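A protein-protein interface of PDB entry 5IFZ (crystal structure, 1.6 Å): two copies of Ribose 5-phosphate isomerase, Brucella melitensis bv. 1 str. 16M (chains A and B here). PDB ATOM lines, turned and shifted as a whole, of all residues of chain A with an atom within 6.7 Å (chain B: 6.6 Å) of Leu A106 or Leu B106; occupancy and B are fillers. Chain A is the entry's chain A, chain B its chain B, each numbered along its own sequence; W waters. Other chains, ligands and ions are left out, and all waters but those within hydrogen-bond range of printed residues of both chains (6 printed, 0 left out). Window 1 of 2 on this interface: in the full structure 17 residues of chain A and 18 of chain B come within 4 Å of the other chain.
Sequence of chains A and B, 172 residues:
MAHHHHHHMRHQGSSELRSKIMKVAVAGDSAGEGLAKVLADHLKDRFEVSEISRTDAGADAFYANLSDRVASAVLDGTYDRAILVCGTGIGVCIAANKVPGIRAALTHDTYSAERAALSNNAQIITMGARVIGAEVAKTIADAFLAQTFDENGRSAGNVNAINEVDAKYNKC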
ATOM      1  N   THR A  88      16.013  -1.280 -16.592  1.00  0.00           N
ATOM      2  CA  THR A  88      16.757  -2.483 -16.231  1.00  0.00           C
ATOM      3  C   THR A  88      18.218  -2.220 -15.912  1.00  0.00           C
ATOM      4  O   THR A  88      18.850  -3.062 -15.269  1.00  0.00           O
ATOM      5  CB  THR A  88      16.721  -3.519 -17.369  1.00  0.00           C
ATOM      6  OG1 THR A  88      17.390  -2.975 -18.518  1.00  0.00           O
ATOM      7  CG2 THR A  88      15.282  -3.906 -17.734  1.00  0.00           C
ATOM      8  N   GLY A  89      18.767  -1.094 -16.362  1.00  0.00           N
ATOM      9  CA  GLY A  89      20.196  -0.843 -16.282  1.00  0.00           C
ATOM     10  C   GLY A  89      20.989  -1.325 -17.479  1.00  0.00           C
ATOM     11  O   GLY A  89      22.168  -0.957 -17.619  1.00  0.00           O
ATOM     12  N   ILE A  90      20.377  -2.105 -18.368  1.00  0.00           N
ATOM     13  CA  ILE A  90      21.117  -2.721 -19.466  1.00  0.00           C
ATOM     14  C   ILE A  90      21.501  -1.687 -20.515  1.00  0.00           C
ATOM     15  O   ILE A  90      22.653  -1.644 -20.968  1.00  0.00           O
ATOM     16  CB  ILE A  90      20.292  -3.861 -20.086  1.00  0.00           C
ATOM     17  CG1 ILE A  90      20.145  -4.997 -19.076  1.00  0.00           C
ATOM     18  CG2 ILE A  90      20.954  -4.344 -21.361  1.00  0.00           C
ATOM     19  CD1 ILE A  90      19.076  -6.044 -19.488  1.00  0.00           C
ATOM     20  N   GLY A  91      20.540  -0.864 -20.948  1.00  0.00           N
ATOM     21  CA  GLY A  91      20.814   0.050 -22.049  1.00  0.00           C
ATOM     22  C   GLY A  91      21.856   1.097 -21.703  1.00  0.00           C
ATOM     23  O   GLY A  91      22.727   1.411 -22.521  1.00  0.00           O
ATOM     24  N   CYS A  93      24.166   0.746 -19.517  1.00  0.00           N
ATOM     25  CA  CYS A  93      25.433   0.034 -19.401  1.00  0.00           C
ATOM     26  C   CYS A  93      26.066  -0.175 -20.772  1.00  0.00           C
ATOM     27  O   CYS A  93      27.256   0.103 -20.966  1.00  0.00           O
ATOM     28  CB  CYS A  93      25.207  -1.301 -18.687  1.00  0.00           C
ATOM     29  SG  CYS A  93      26.714  -2.281 -18.489  1.00  0.00           S
ATOM     30  N   ASN A  97      29.623   1.846 -21.899  1.00  0.00           N
ATOM     31  CA  ASN A  97      30.825   1.102 -22.263  1.00  0.00           C
ATOM     32  C   ASN A  97      31.272   1.377 -23.689  1.00  0.00           C
ATOM     33  O   ASN A  97      32.442   1.144 -24.019  1.00  0.00           O
ATOM     34  CB  ASN A  97      30.590  -0.391 -22.050  1.00  0.00           C
ATOM     35  CG  ASN A  97      30.755  -0.787 -20.607  1.00  0.00           C
ATOM     36  OD1 ASN A  97      31.767  -0.476 -19.988  1.00  0.00           O
ATOM     37  ND2 ASN A  97      29.750  -1.451 -20.049  1.00  0.00           N
ATOM     38  N   ALA A 104      31.634   0.650 -17.382  1.00  0.00           N
ATOM     39  CA  ALA A 104      30.348   0.715 -16.699  1.00  0.00           C
ATOM     40  C   ALA A 104      29.887  -0.683 -16.298  1.00  0.00           C
ATOM     41  O   ALA A 104      29.980  -1.634 -17.081  1.00  0.00           O
ATOM     42  CB  ALA A 104      29.281   1.385 -17.581  1.00  0.00           C
ATOM     43  N   ALA A 105      29.395  -0.796 -15.073  1.00  0.00           N
ATOM     44  CA  ALA A 105      28.983  -2.074 -14.501  1.00  0.00           C
ATOM     45  C   ALA A 105      27.534  -1.988 -14.056  1.00  0.00           C
ATOM     46  O   ALA A 105      27.166  -1.095 -13.293  1.00  0.00           O
ATOM     47  CB  ALA A 105      29.872  -2.445 -13.318  1.00  0.00           C
ATOM     48  N   LEU A 106      26.718  -2.929 -14.522  1.00  0.00           N
ATOM     49  CA  LEU A 106      25.364  -3.068 -14.008  1.00  0.00           C
ATOM     50  C   LEU A 106      25.466  -3.833 -12.693  1.00  0.00           C
ATOM     51  O   LEU A 106      25.917  -4.981 -12.684  1.00  0.00           O
ATOM     52  CB  LEU A 106      24.496  -3.814 -15.019  1.00  0.00           C
ATOM     53  CG  LEU A 106      22.975  -3.878 -14.799  1.00  0.00           C
ATOM     54  CD1 LEU A 106      22.304  -4.422 -16.053  1.00  0.00           C
ATOM     55  CD2 LEU A 106      22.593  -4.729 -13.616  1.00  0.00           C
ATOM     56  N   THR A 107      25.070  -3.204 -11.585  1.00  0.00           N
ATOM     57  CA  THR A 107      25.311  -3.764 -10.255  1.00  0.00           C
ATOM     58  C   THR A 107      23.984  -3.911  -9.519  1.00  0.00           C
ATOM     59  O   THR A 107      23.395  -2.916  -9.089  1.00  0.00           O
ATOM     60  CB  THR A 107      26.271  -2.882  -9.455  1.00  0.00           C
ATOM     61  OG1 THR A 107      25.763  -1.546  -9.417  1.00  0.00           O
ATOM     62  CG2 THR A 107      27.642  -2.895 -10.119  1.00  0.00           C
ATOM     63  N   HIS A 108      23.530  -5.153  -9.338  1.00  0.00           N
ATOM     64  CA  HIS A 108      22.265  -5.393  -8.644  1.00  0.00           C
ATOM     65  C   HIS A 108      22.447  -6.162  -7.337  1.00  0.00           C
ATOM     66  O   HIS A 108      21.476  -6.709  -6.793  1.00  0.00           O
ATOM     67  CB  HIS A 108      21.267  -6.091  -9.580  1.00  0.00           C
ATOM     68  CG  HIS A 108      20.536  -5.135 -10.471  1.00  0.00           C
ATOM     69  ND1 HIS A 108      19.699  -5.545 -11.485  1.00  0.00           N
ATOM     70  CD2 HIS A 108      20.532  -3.779 -10.505  1.00  0.00           C
ATOM     71  CE1 HIS A 108      19.209  -4.483 -12.107  1.00  0.00           C
ATOM     72  NE2 HIS A 108      19.690  -3.399 -11.525  1.00  0.00           N
ATOM     73  N   ASP A 109      23.656  -6.157  -6.781  1.00  0.00           N
ATOM     74  CA  ASP A 109      23.934  -6.701  -5.462  1.00  0.00           C
ATOM     75  C   ASP A 109      25.206  -6.035  -4.955  1.00  0.00           C
ATOM     76  O   ASP A 109      26.000  -5.512  -5.742  1.00  0.00           O
ATOM     77  CB  ASP A 109      24.092  -8.224  -5.493  1.00  0.00           C
ATOM     78  CG  ASP A 109      25.295  -8.666  -6.302  1.00  0.00           C
ATOM     79  OD1 ASP A 109      25.183  -8.855  -7.530  1.00  0.00           O
ATOM     80  OD2 ASP A 109      26.366  -8.815  -5.701  1.00  0.00           O
ATOM     81  N   SER A 112      28.695  -7.514  -6.246  1.00  0.00           N
ATOM     82  CA  SER A 112      29.042  -7.033  -7.580  1.00  0.00           C
ATOM     83  C   SER A 112      29.407  -5.559  -7.562  1.00  0.00           C
ATOM     84  O   SER A 112      30.235  -5.127  -8.363  1.00  0.00           O
ATOM     85  CB  SER A 112      27.887  -7.267  -8.552  1.00  0.00           C
ATOM     86  OG  SER A 112      27.534  -8.646  -8.596  1.00  0.00           O
ATOM     87  N   ALA A 113      28.756  -4.770  -6.703  1.00  0.00           N
ATOM     88  CA  ALA A 113      29.093  -3.352  -6.607  1.00  0.00           C
ATOM     89  C   ALA A 113      30.534  -3.169  -6.154  1.00  0.00           C
ATOM     90  O   ALA A 113      31.267  -2.343  -6.714  1.00  0.00           O
ATOM     91  CB  ALA A 113      28.130  -2.648  -5.648  1.00  0.00           C
ATOM     92  N   ALA A 116      32.778  -4.191  -9.020  1.00  0.00           N
ATOM     93  CA  ALA A 116      32.815  -3.199 -10.090  1.00  0.00           C
ATOM     94  C   ALA A 116      33.946  -2.214  -9.861  1.00  0.00           C
ATOM     95  O   ALA A 116      34.670  -1.860 -10.797  1.00  0.00           O
ATOM     96  CB  ALA A 116      31.481  -2.456 -10.169  1.00  0.00           C
ATOM     97  N   ILE A 124      31.493   4.023 -13.560  1.00  0.00           N
ATOM     98  CA  ILE A 124      30.044   4.162 -13.603  1.00  0.00           C
ATOM     99  C   ILE A 124      29.413   2.838 -13.203  1.00  0.00           C
ATOM    100  O   ILE A 124      29.850   1.775 -13.657  1.00  0.00           O
ATOM    101  CB  ILE A 124      29.574   4.578 -15.012  1.00  0.00           C
ATOM    102  CG1 ILE A 124      30.129   5.964 -15.370  1.00  0.00           C
ATOM    103  CG2 ILE A 124      28.049   4.524 -15.120  1.00  0.00           C
ATOM    104  CD1 ILE A 124      29.772   6.439 -16.775  1.00  0.00           C
ATOM    105  N   ILE A 125      28.387   2.900 -12.359  1.00  0.00           N
ATOM    106  CA  ILE A 125      27.531   1.743 -12.120  1.00  0.00           C
ATOM    107  C   ILE A 125      26.130   2.076 -12.616  1.00  0.00           C
ATOM    108  O   ILE A 125      25.729   3.243 -12.670  1.00  0.00           O
ATOM    109  CB  ILE A 125      27.503   1.297 -10.641  1.00  0.00           C
ATOM    110  CG1 ILE A 125      26.963   2.414  -9.736  1.00  0.00           C
ATOM    111  CG2 ILE A 125      28.903   0.835 -10.197  1.00  0.00           C
ATOM    112  CD1 ILE A 125      26.624   1.947  -8.314  1.00  0.00           C
ATOM    113  N   THR A 126      25.390   1.042 -13.012  1.00  0.00           N
ATOM    114  CA  THR A 126      24.031   1.234 -13.501  1.00  0.00           C
ATOM    115  C   THR A 126      23.091   0.316 -12.734  1.00  0.00           C
ATOM    116  O   THR A 126      23.505  -0.724 -12.230  1.00  0.00           O
ATOM    117  CB  THR A 126      23.900   0.962 -15.023  1.00  0.00           C
ATOM    118  OG1 THR A 126      23.902  -0.446 -15.282  1.00  0.00           O
ATOM    119  CG2 THR A 126      25.049   1.628 -15.809  1.00  0.00           C
ATOM    120  N   MET A 127      21.830   0.726 -12.641  1.00  0.00           N
ATOM    121  CA  MET A 127      20.806  -0.020 -11.917  1.00  0.00           C
ATOM    122  C   MET A 127      19.490   0.077 -12.660  1.00  0.00           C
ATOM    123  O   MET A 127      19.241   1.051 -13.373  1.00  0.00           O
ATOM    124  CB  MET A 127      20.558   0.515 -10.509  1.00  0.00           C
ATOM    125  CG  MET A 127      21.758   0.756  -9.686  1.00  0.00           C
ATOM    126  SD  MET A 127      21.206   1.300  -8.071  1.00  0.00           S
ATOM    127  CE  MET A 127      22.763   1.776  -7.368  1.00  0.00           C
ATOM    128  N   GLY A 128      18.622  -0.912 -12.436  1.00  0.00           N
ATOM    129  CA  GLY A 128      17.293  -0.915 -13.009  1.00  0.00           C
ATOM    130  C   GLY A 128      16.216  -0.665 -11.966  1.00  0.00           C
ATOM    131  O   GLY A 128      15.992  -1.494 -11.074  1.00  0.00           O
ATOM    132  N   THR B  88      31.274 -12.427 -11.852  1.00  0.00           N
ATOM    133  CA  THR B  88      30.133 -11.534 -11.694  1.00  0.00           C
ATOM    134  C   THR B  88      29.411 -11.251 -12.995  1.00  0.00           C
ATOM    135  O   THR B  88      28.253 -10.821 -12.959  1.00  0.00           O
ATOM    136  CB  THR B  88      30.560 -10.174 -11.119  1.00  0.00           C
ATOM    137  OG1 THR B  88      31.336  -9.477 -12.104  1.00  0.00           O
ATOM    138  CG2 THR B  88      31.377 -10.353  -9.848  1.00  0.00           C
ATOM    139  N   GLY B  89      30.071 -11.451 -14.133  1.00  0.00           N
ATOM    140  CA  GLY B  89      29.515 -11.075 -15.410  1.00  0.00           C
ATOM    141  C   GLY B  89      29.841  -9.660 -15.834  1.00  0.00           C
ATOM    142  O   GLY B  89      29.539  -9.289 -16.973  1.00  0.00           O
ATOM    143  N   ILE B  90      30.470  -8.868 -14.961  1.00  0.00           N
ATOM    144  CA  ILE B  90      30.731  -7.466 -15.276  1.00  0.00           C
ATOM    145  C   ILE B  90      31.839  -7.343 -16.310  1.00  0.00           C
ATOM    146  O   ILE B  90      31.688  -6.644 -17.320  1.00  0.00           O
ATOM    147  CB  ILE B  90      31.076  -6.686 -13.998  1.00  0.00           C
ATOM    148  CG1 ILE B  90      29.846  -6.633 -13.078  1.00  0.00           C
ATOM    149  CG2 ILE B  90      31.607  -5.292 -14.360  1.00  0.00           C
ATOM    150  CD1 ILE B  90      30.172  -6.058 -11.703  1.00  0.00           C
ATOM    151  N   GLY B  91      32.982  -7.996 -16.060  1.00  0.00           N
ATOM    152  CA  GLY B  91      34.128  -7.836 -16.944  1.00  0.00           C
ATOM    153  C   GLY B  91      33.845  -8.264 -18.372  1.00  0.00           C
ATOM    154  O   GLY B  91      34.267  -7.602 -19.323  1.00  0.00           O
ATOM    155  N   CYS B  93      30.931  -8.344 -19.781  1.00  0.00           N
ATOM    156  CA  CYS B  93      29.967  -7.417 -20.355  1.00  0.00           C
ATOM    157  C   CYS B  93      30.663  -6.164 -20.870  1.00  0.00           C
ATOM    158  O   CYS B  93      30.405  -5.725 -21.995  1.00  0.00           O
ATOM    159  CB  CYS B  93      28.891  -7.068 -19.323  1.00  0.00           C
ATOM    160  SG  CYS B  93      27.620  -5.933 -19.928  1.00  0.00           S
ATOM    161  N   ASN B  97      30.920  -5.305 -24.967  1.00  0.00           N
ATOM    162  CA  ASN B  97      30.342  -4.066 -25.473  1.00  0.00           C
ATOM    163  C   ASN B  97      31.373  -3.157 -26.145  1.00  0.00           C
ATOM    164  O   ASN B  97      30.990  -2.305 -26.962  1.00  0.00           O
ATOM    165  CB  ASN B  97      29.620  -3.345 -24.338  1.00  0.00           C
ATOM    166  CG  ASN B  97      28.215  -3.863 -24.148  1.00  0.00           C
ATOM    167  OD1 ASN B  97      27.468  -3.965 -25.118  1.00  0.00           O
ATOM    168  ND2 ASN B  97      27.847  -4.194 -22.908  1.00  0.00           N
ATOM    169  N   ALA B 104      25.880  -6.355 -25.427  1.00  0.00           N
ATOM    170  CA  ALA B 104      25.936  -7.389 -24.403  1.00  0.00           C
ATOM    171  C   ALA B 104      25.224  -6.924 -23.140  1.00  0.00           C
ATOM    172  O   ALA B 104      25.364  -5.773 -22.718  1.00  0.00           O
ATOM    173  CB  ALA B 104      27.391  -7.774 -24.089  1.00  0.00           C
ATOM    174  N   ALA B 105      24.438  -7.819 -22.545  1.00  0.00           N
ATOM    175  CA  ALA B 105      23.622  -7.503 -21.383  1.00  0.00           C
ATOM    176  C   ALA B 105      23.989  -8.439 -20.243  1.00  0.00           C
ATOM    177  O   ALA B 105      23.897  -9.659 -20.397  1.00  0.00           O
ATOM    178  CB  ALA B 105      22.136  -7.656 -21.730  1.00  0.00           C
ATOM    179  N   LEU B 106      24.356  -7.880 -19.089  1.00  0.00           N
ATOM    180  CA  LEU B 106      24.438  -8.684 -17.873  1.00  0.00           C
ATOM    181  C   LEU B 106      23.015  -8.923 -17.371  1.00  0.00           C
ATOM    182  O   LEU B 106      22.310  -7.971 -17.021  1.00  0.00           O
ATOM    183  CB  LEU B 106      25.283  -7.977 -16.810  1.00  0.00           C
ATOM    184  CG  LEU B 106      25.721  -8.763 -15.559  1.00  0.00           C
ATOM    185  CD1 LEU B 106      26.822  -8.010 -14.827  1.00  0.00           C
ATOM    186  CD2 LEU B 106      24.585  -9.031 -14.587  1.00  0.00           C
ATOM    187  N   THR B 107      22.593 -10.185 -17.334  1.00  0.00           N
ATOM    188  CA  THR B 107      21.207 -10.538 -17.012  1.00  0.00           C
ATOM    189  C   THR B 107      21.163 -11.461 -15.798  1.00  0.00           C
ATOM    190  O   THR B 107      21.508 -12.643 -15.900  1.00  0.00           O
ATOM    191  CB  THR B 107      20.542 -11.221 -18.207  1.00  0.00           C
ATOM    192  OG1 THR B 107      21.312 -12.365 -18.588  1.00  0.00           O
ATOM    193  CG2 THR B 107      20.431 -10.260 -19.383  1.00  0.00           C
ATOM    194  N   HIS B 108      20.689 -10.941 -14.657  1.00  0.00           N
ATOM    195  CA  HIS B 108      20.599 -11.757 -13.451  1.00  0.00           C
ATOM    196  C   HIS B 108      19.167 -11.955 -12.990  1.00  0.00           C
ATOM    197  O   HIS B 108      18.936 -12.371 -11.847  1.00  0.00           O
ATOM    198  CB  HIS B 108      21.463 -11.172 -12.336  1.00  0.00           C
ATOM    199  CG  HIS B 108      22.896 -11.585 -12.443  1.00  0.00           C
ATOM    200  ND1 HIS B 108      23.886 -11.080 -11.625  1.00  0.00           N
ATOM    201  CD2 HIS B 108      23.507 -12.464 -13.277  1.00  0.00           C
ATOM    202  CE1 HIS B 108      25.043 -11.631 -11.950  1.00  0.00           C
ATOM    203  NE2 HIS B 108      24.843 -12.473 -12.949  1.00  0.00           N
ATOM    204  N   ASP B 109      18.203 -11.740 -13.877  1.00  0.00           N
ATOM    205  CA  ASP B 109      16.818 -12.083 -13.584  1.00  0.00           C
ATOM    206  C   ASP B 109      16.097 -12.287 -14.909  1.00  0.00           C
ATOM    207  O   ASP B 109      16.545 -11.813 -15.957  1.00  0.00           O
ATOM    208  CB  ASP B 109      16.138 -10.999 -12.736  1.00  0.00           C
ATOM    209  CG  ASP B 109      15.946  -9.713 -13.498  1.00  0.00           C
ATOM    210  OD1 ASP B 109      14.901  -9.566 -14.157  1.00  0.00           O
ATOM    211  OD2 ASP B 109      16.850  -8.850 -13.462  1.00  0.00           O
ATOM    212  N   SER B 112      14.816  -9.073 -16.850  1.00  0.00           N
ATOM    213  CA  SER B 112      15.912  -8.424 -17.562  1.00  0.00           C
ATOM    214  C   SER B 112      16.378  -9.246 -18.752  1.00  0.00           C
ATOM    215  O   SER B 112      16.756  -8.677 -19.789  1.00  0.00           O
ATOM    216  CB  SER B 112      17.066  -8.179 -16.597  1.00  0.00           C
ATOM    217  OG  SER B 112      16.667  -7.250 -15.605  1.00  0.00           O
ATOM    218  N   ILE B 124      24.466 -11.068 -26.964  1.00  0.00           N
ATOM    219  CA  ILE B 124      25.219 -11.749 -25.920  1.00  0.00           C
ATOM    220  C   ILE B 124      24.632 -11.362 -24.572  1.00  0.00           C
ATOM    221  O   ILE B 124      24.381 -10.178 -24.316  1.00  0.00           O
ATOM    222  CB  ILE B 124      26.718 -11.383 -25.968  1.00  0.00           C
ATOM    223  CG1 ILE B 124      27.333 -11.793 -27.315  1.00  0.00           C
ATOM    224  CG2 ILE B 124      27.456 -12.023 -24.796  1.00  0.00           C
ATOM    225  CD1 ILE B 124      28.810 -11.435 -27.466  1.00  0.00           C
ATOM    226  N   ILE B 125      24.417 -12.352 -23.713  1.00  0.00           N
ATOM    227  CA  ILE B 125      24.099 -12.091 -22.319  1.00  0.00           C
ATOM    228  C   ILE B 125      25.240 -12.629 -21.477  1.00  0.00           C
ATOM    229  O   ILE B 125      25.946 -13.561 -21.878  1.00  0.00           O
ATOM    230  CB  ILE B 125      22.750 -12.693 -21.868  1.00  0.00           C
ATOM    231  CG1 ILE B 125      22.719 -14.210 -22.078  1.00  0.00           C
ATOM    232  CG2 ILE B 125      21.606 -12.008 -22.602  1.00  0.00           C
ATOM    233  CD1 ILE B 125      21.506 -14.867 -21.419  1.00  0.00           C
ATOM    234  N   THR B 126      25.443 -12.014 -20.315  1.00  0.00           N
ATOM    235  CA  THR B 126      26.492 -12.451 -19.407  1.00  0.00           C
ATOM    236  C   THR B 126      25.909 -12.689 -18.024  1.00  0.00           C
ATOM    237  O   THR B 126      24.873 -12.124 -17.654  1.00  0.00           O
ATOM    238  CB  THR B 126      27.674 -11.443 -19.327  1.00  0.00           C
ATOM    239  OG1 THR B 126      27.312 -10.295 -18.546  1.00  0.00           O
ATOM    240  CG2 THR B 126      28.099 -10.993 -20.728  1.00  0.00           C
ATOM    241  N   MET B 127      26.568 -13.571 -17.280  1.00  0.00           N
ATOM    242  CA  MET B 127      26.130 -13.954 -15.946  1.00  0.00           C
ATOM    243  C   MET B 127      27.344 -14.159 -15.062  1.00  0.00           C
ATOM    244  O   MET B 127      28.444 -14.435 -15.548  1.00  0.00           O
ATOM    245  CB  MET B 127      25.323 -15.255 -15.937  1.00  0.00           C
ATOM    246  CG  MET B 127      24.360 -15.432 -17.078  1.00  0.00           C
ATOM    247  SD  MET B 127      23.551 -17.024 -16.941  1.00  0.00           S
ATOM    248  CE  MET B 127      22.423 -16.924 -18.323  1.00  0.00           C
ATOM    249  N   GLY B 128      27.113 -14.075 -13.755  1.00  0.00           N
ATOM    250  CA  GLY B 128      28.151 -14.298 -12.774  1.00  0.00           C
ATOM    251  C   GLY B 128      27.935 -15.562 -11.975  1.00  0.00           C
ATOM    252  O   GLY B 128      27.006 -15.644 -11.167  1.00  0.00           O
HETATM  253  O   HOH W   1      23.259  -9.212  -9.469  1.00  0.00           O
HETATM  254  O   HOH W   2      18.847  -5.883 -14.844  1.00  0.00           O
HETATM  255  O   HOH W   3      24.467  -4.195 -20.408  1.00  0.00           O
HETATM  256  O   HOH W   4      29.308  -4.484 -17.375  1.00  0.00           O
HETATM  257  O   HOH W   5      26.829  -9.160 -11.066  1.00  0.00           O
HETATM  258  O   HOH W   6      19.040  -8.412 -11.937  1.00  0.00           O
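The backbone NH (N) of Ala A105 lies within hydrogen-bond range of the backbone carbonyl oxygen (O) of Ile A124. The side-chain hydroxyl (OG) of Ser A112 lies within hydrogen-bond range of the side-chain carboxylate (OD1) of Asp A109 (2.6 Å). The side-chain hydroxyl of Thr B88 lies within hydrogen-bond range of the backbone NH of Ile B90, at 3.0 Å. O of Ile B124 lies within hydrogen-bond range of N of Ala B105 (3.0 Å). The backbone NH (N) of Thr B126 sits at hydrogen-bond distance from the backbone carbonyl oxygen (O) of Ala B105, at 2.8 Å. The side-chain hydroxyl (OG) of Ser B112 is in hydrogen-bond range of the side-chain carboxylate (OD2) of Asp B109, 2.7 Å away.
Of the printed residues of chain B, Ile A90 touches Ala B105 and Ser B112. Printed residues of chain B within 4 Å of Asn A97: Asn B97 (3.9 Å). Cys B93 touches none of the printed residues of chain A. Of the printed residues of chain A, Leu B106 touches Leu A106 (3.7 Å). The nearest residue of chain B that does not touch Leu A106 is Ile B90 (4.3 Å). The nearest residue of chain A that does not touch Leu B106 is Ile A90 (4.2 Å). The nearest printed residue of chain A that does not touch Ala B105 is Leu A106 (6.0 Å).
Ile A90 touches Ala B105, and with the chains exchanged Ala A105 touches Ile B90. Ile A90 touches Ser B112, and with the chains exchanged Ser A112 touches Ile B90. Asn A97 touches its own counterpart, Asn B97. Leu B106 touches its own counterpart, Leu A106. 18 positions are printed for both chains. Of the 6 pairs that touch across the chains among the printed residues, 6 have their exchanged pair printed and touching as well.
Water W5 bridges the side-chain hydroxyl of Ser A112 and the backbone carbonyl oxygen of Thr B88. Water W2 lies within hydrogen-bond range of the side-chain hydroxyl of Ser B112, the backbone carbonyl oxygen of Thr A88 and a ring nitrogen (ND1) of His A108. Water W6 lies within hydrogen-bond range of OD2 of Asp B109 and ND1 of His A108. Water W1 lies within hydrogen-bond range of OD1 of Asp A109 (2.8 Å) and ND1 of His B108 (2.9 Å). Water W3 lies within hydrogen-bond range of the backbone carbonyl oxygen (O) of Ala B104 (2.9 Å), the backbone carbonyl oxygen (O) of Ile A90 (3.2 Å), the side-chain sulfur (SG) of Cys A93 (3.5 Å) and the side-chain sulfur (SG) of Cys B93 (3.6 Å). Water W4 lies within hydrogen-bond range of the backbone carbonyl oxygen of Ala A104 (2.9 Å), the backbone carbonyl oxygen of Ile B90 (3.2 Å), the side-chain sulfur of Cys B93 (3.4 Å) and the side-chain sulfur of Cys A93 (3.6 Å).
Of the 18 printed residues of chain B, 5 touch a printed residue of chain A. Printed residues of chain B that touch a printed residue of chain A: Ile B90, Asn B97, Ala B105, Leu B106 and Ser B112. Among the printed residues, no Asp or Glu carboxylate lies within 4 Å of a Lys or Arg side-chain nitrogen of the other chain.
CG2 of Ile A90 touches CB of Ala B105 (3.5 Å). Ser B112 touches Ile A90. Asn A97 touches Asn B97. Ile B90 touches Ala A105 (CG2 to CB, 3.5 Å). Leu B106 touches Leu A106 (O to CD1, 3.7 Å). Ser A112 touches Ile B90.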
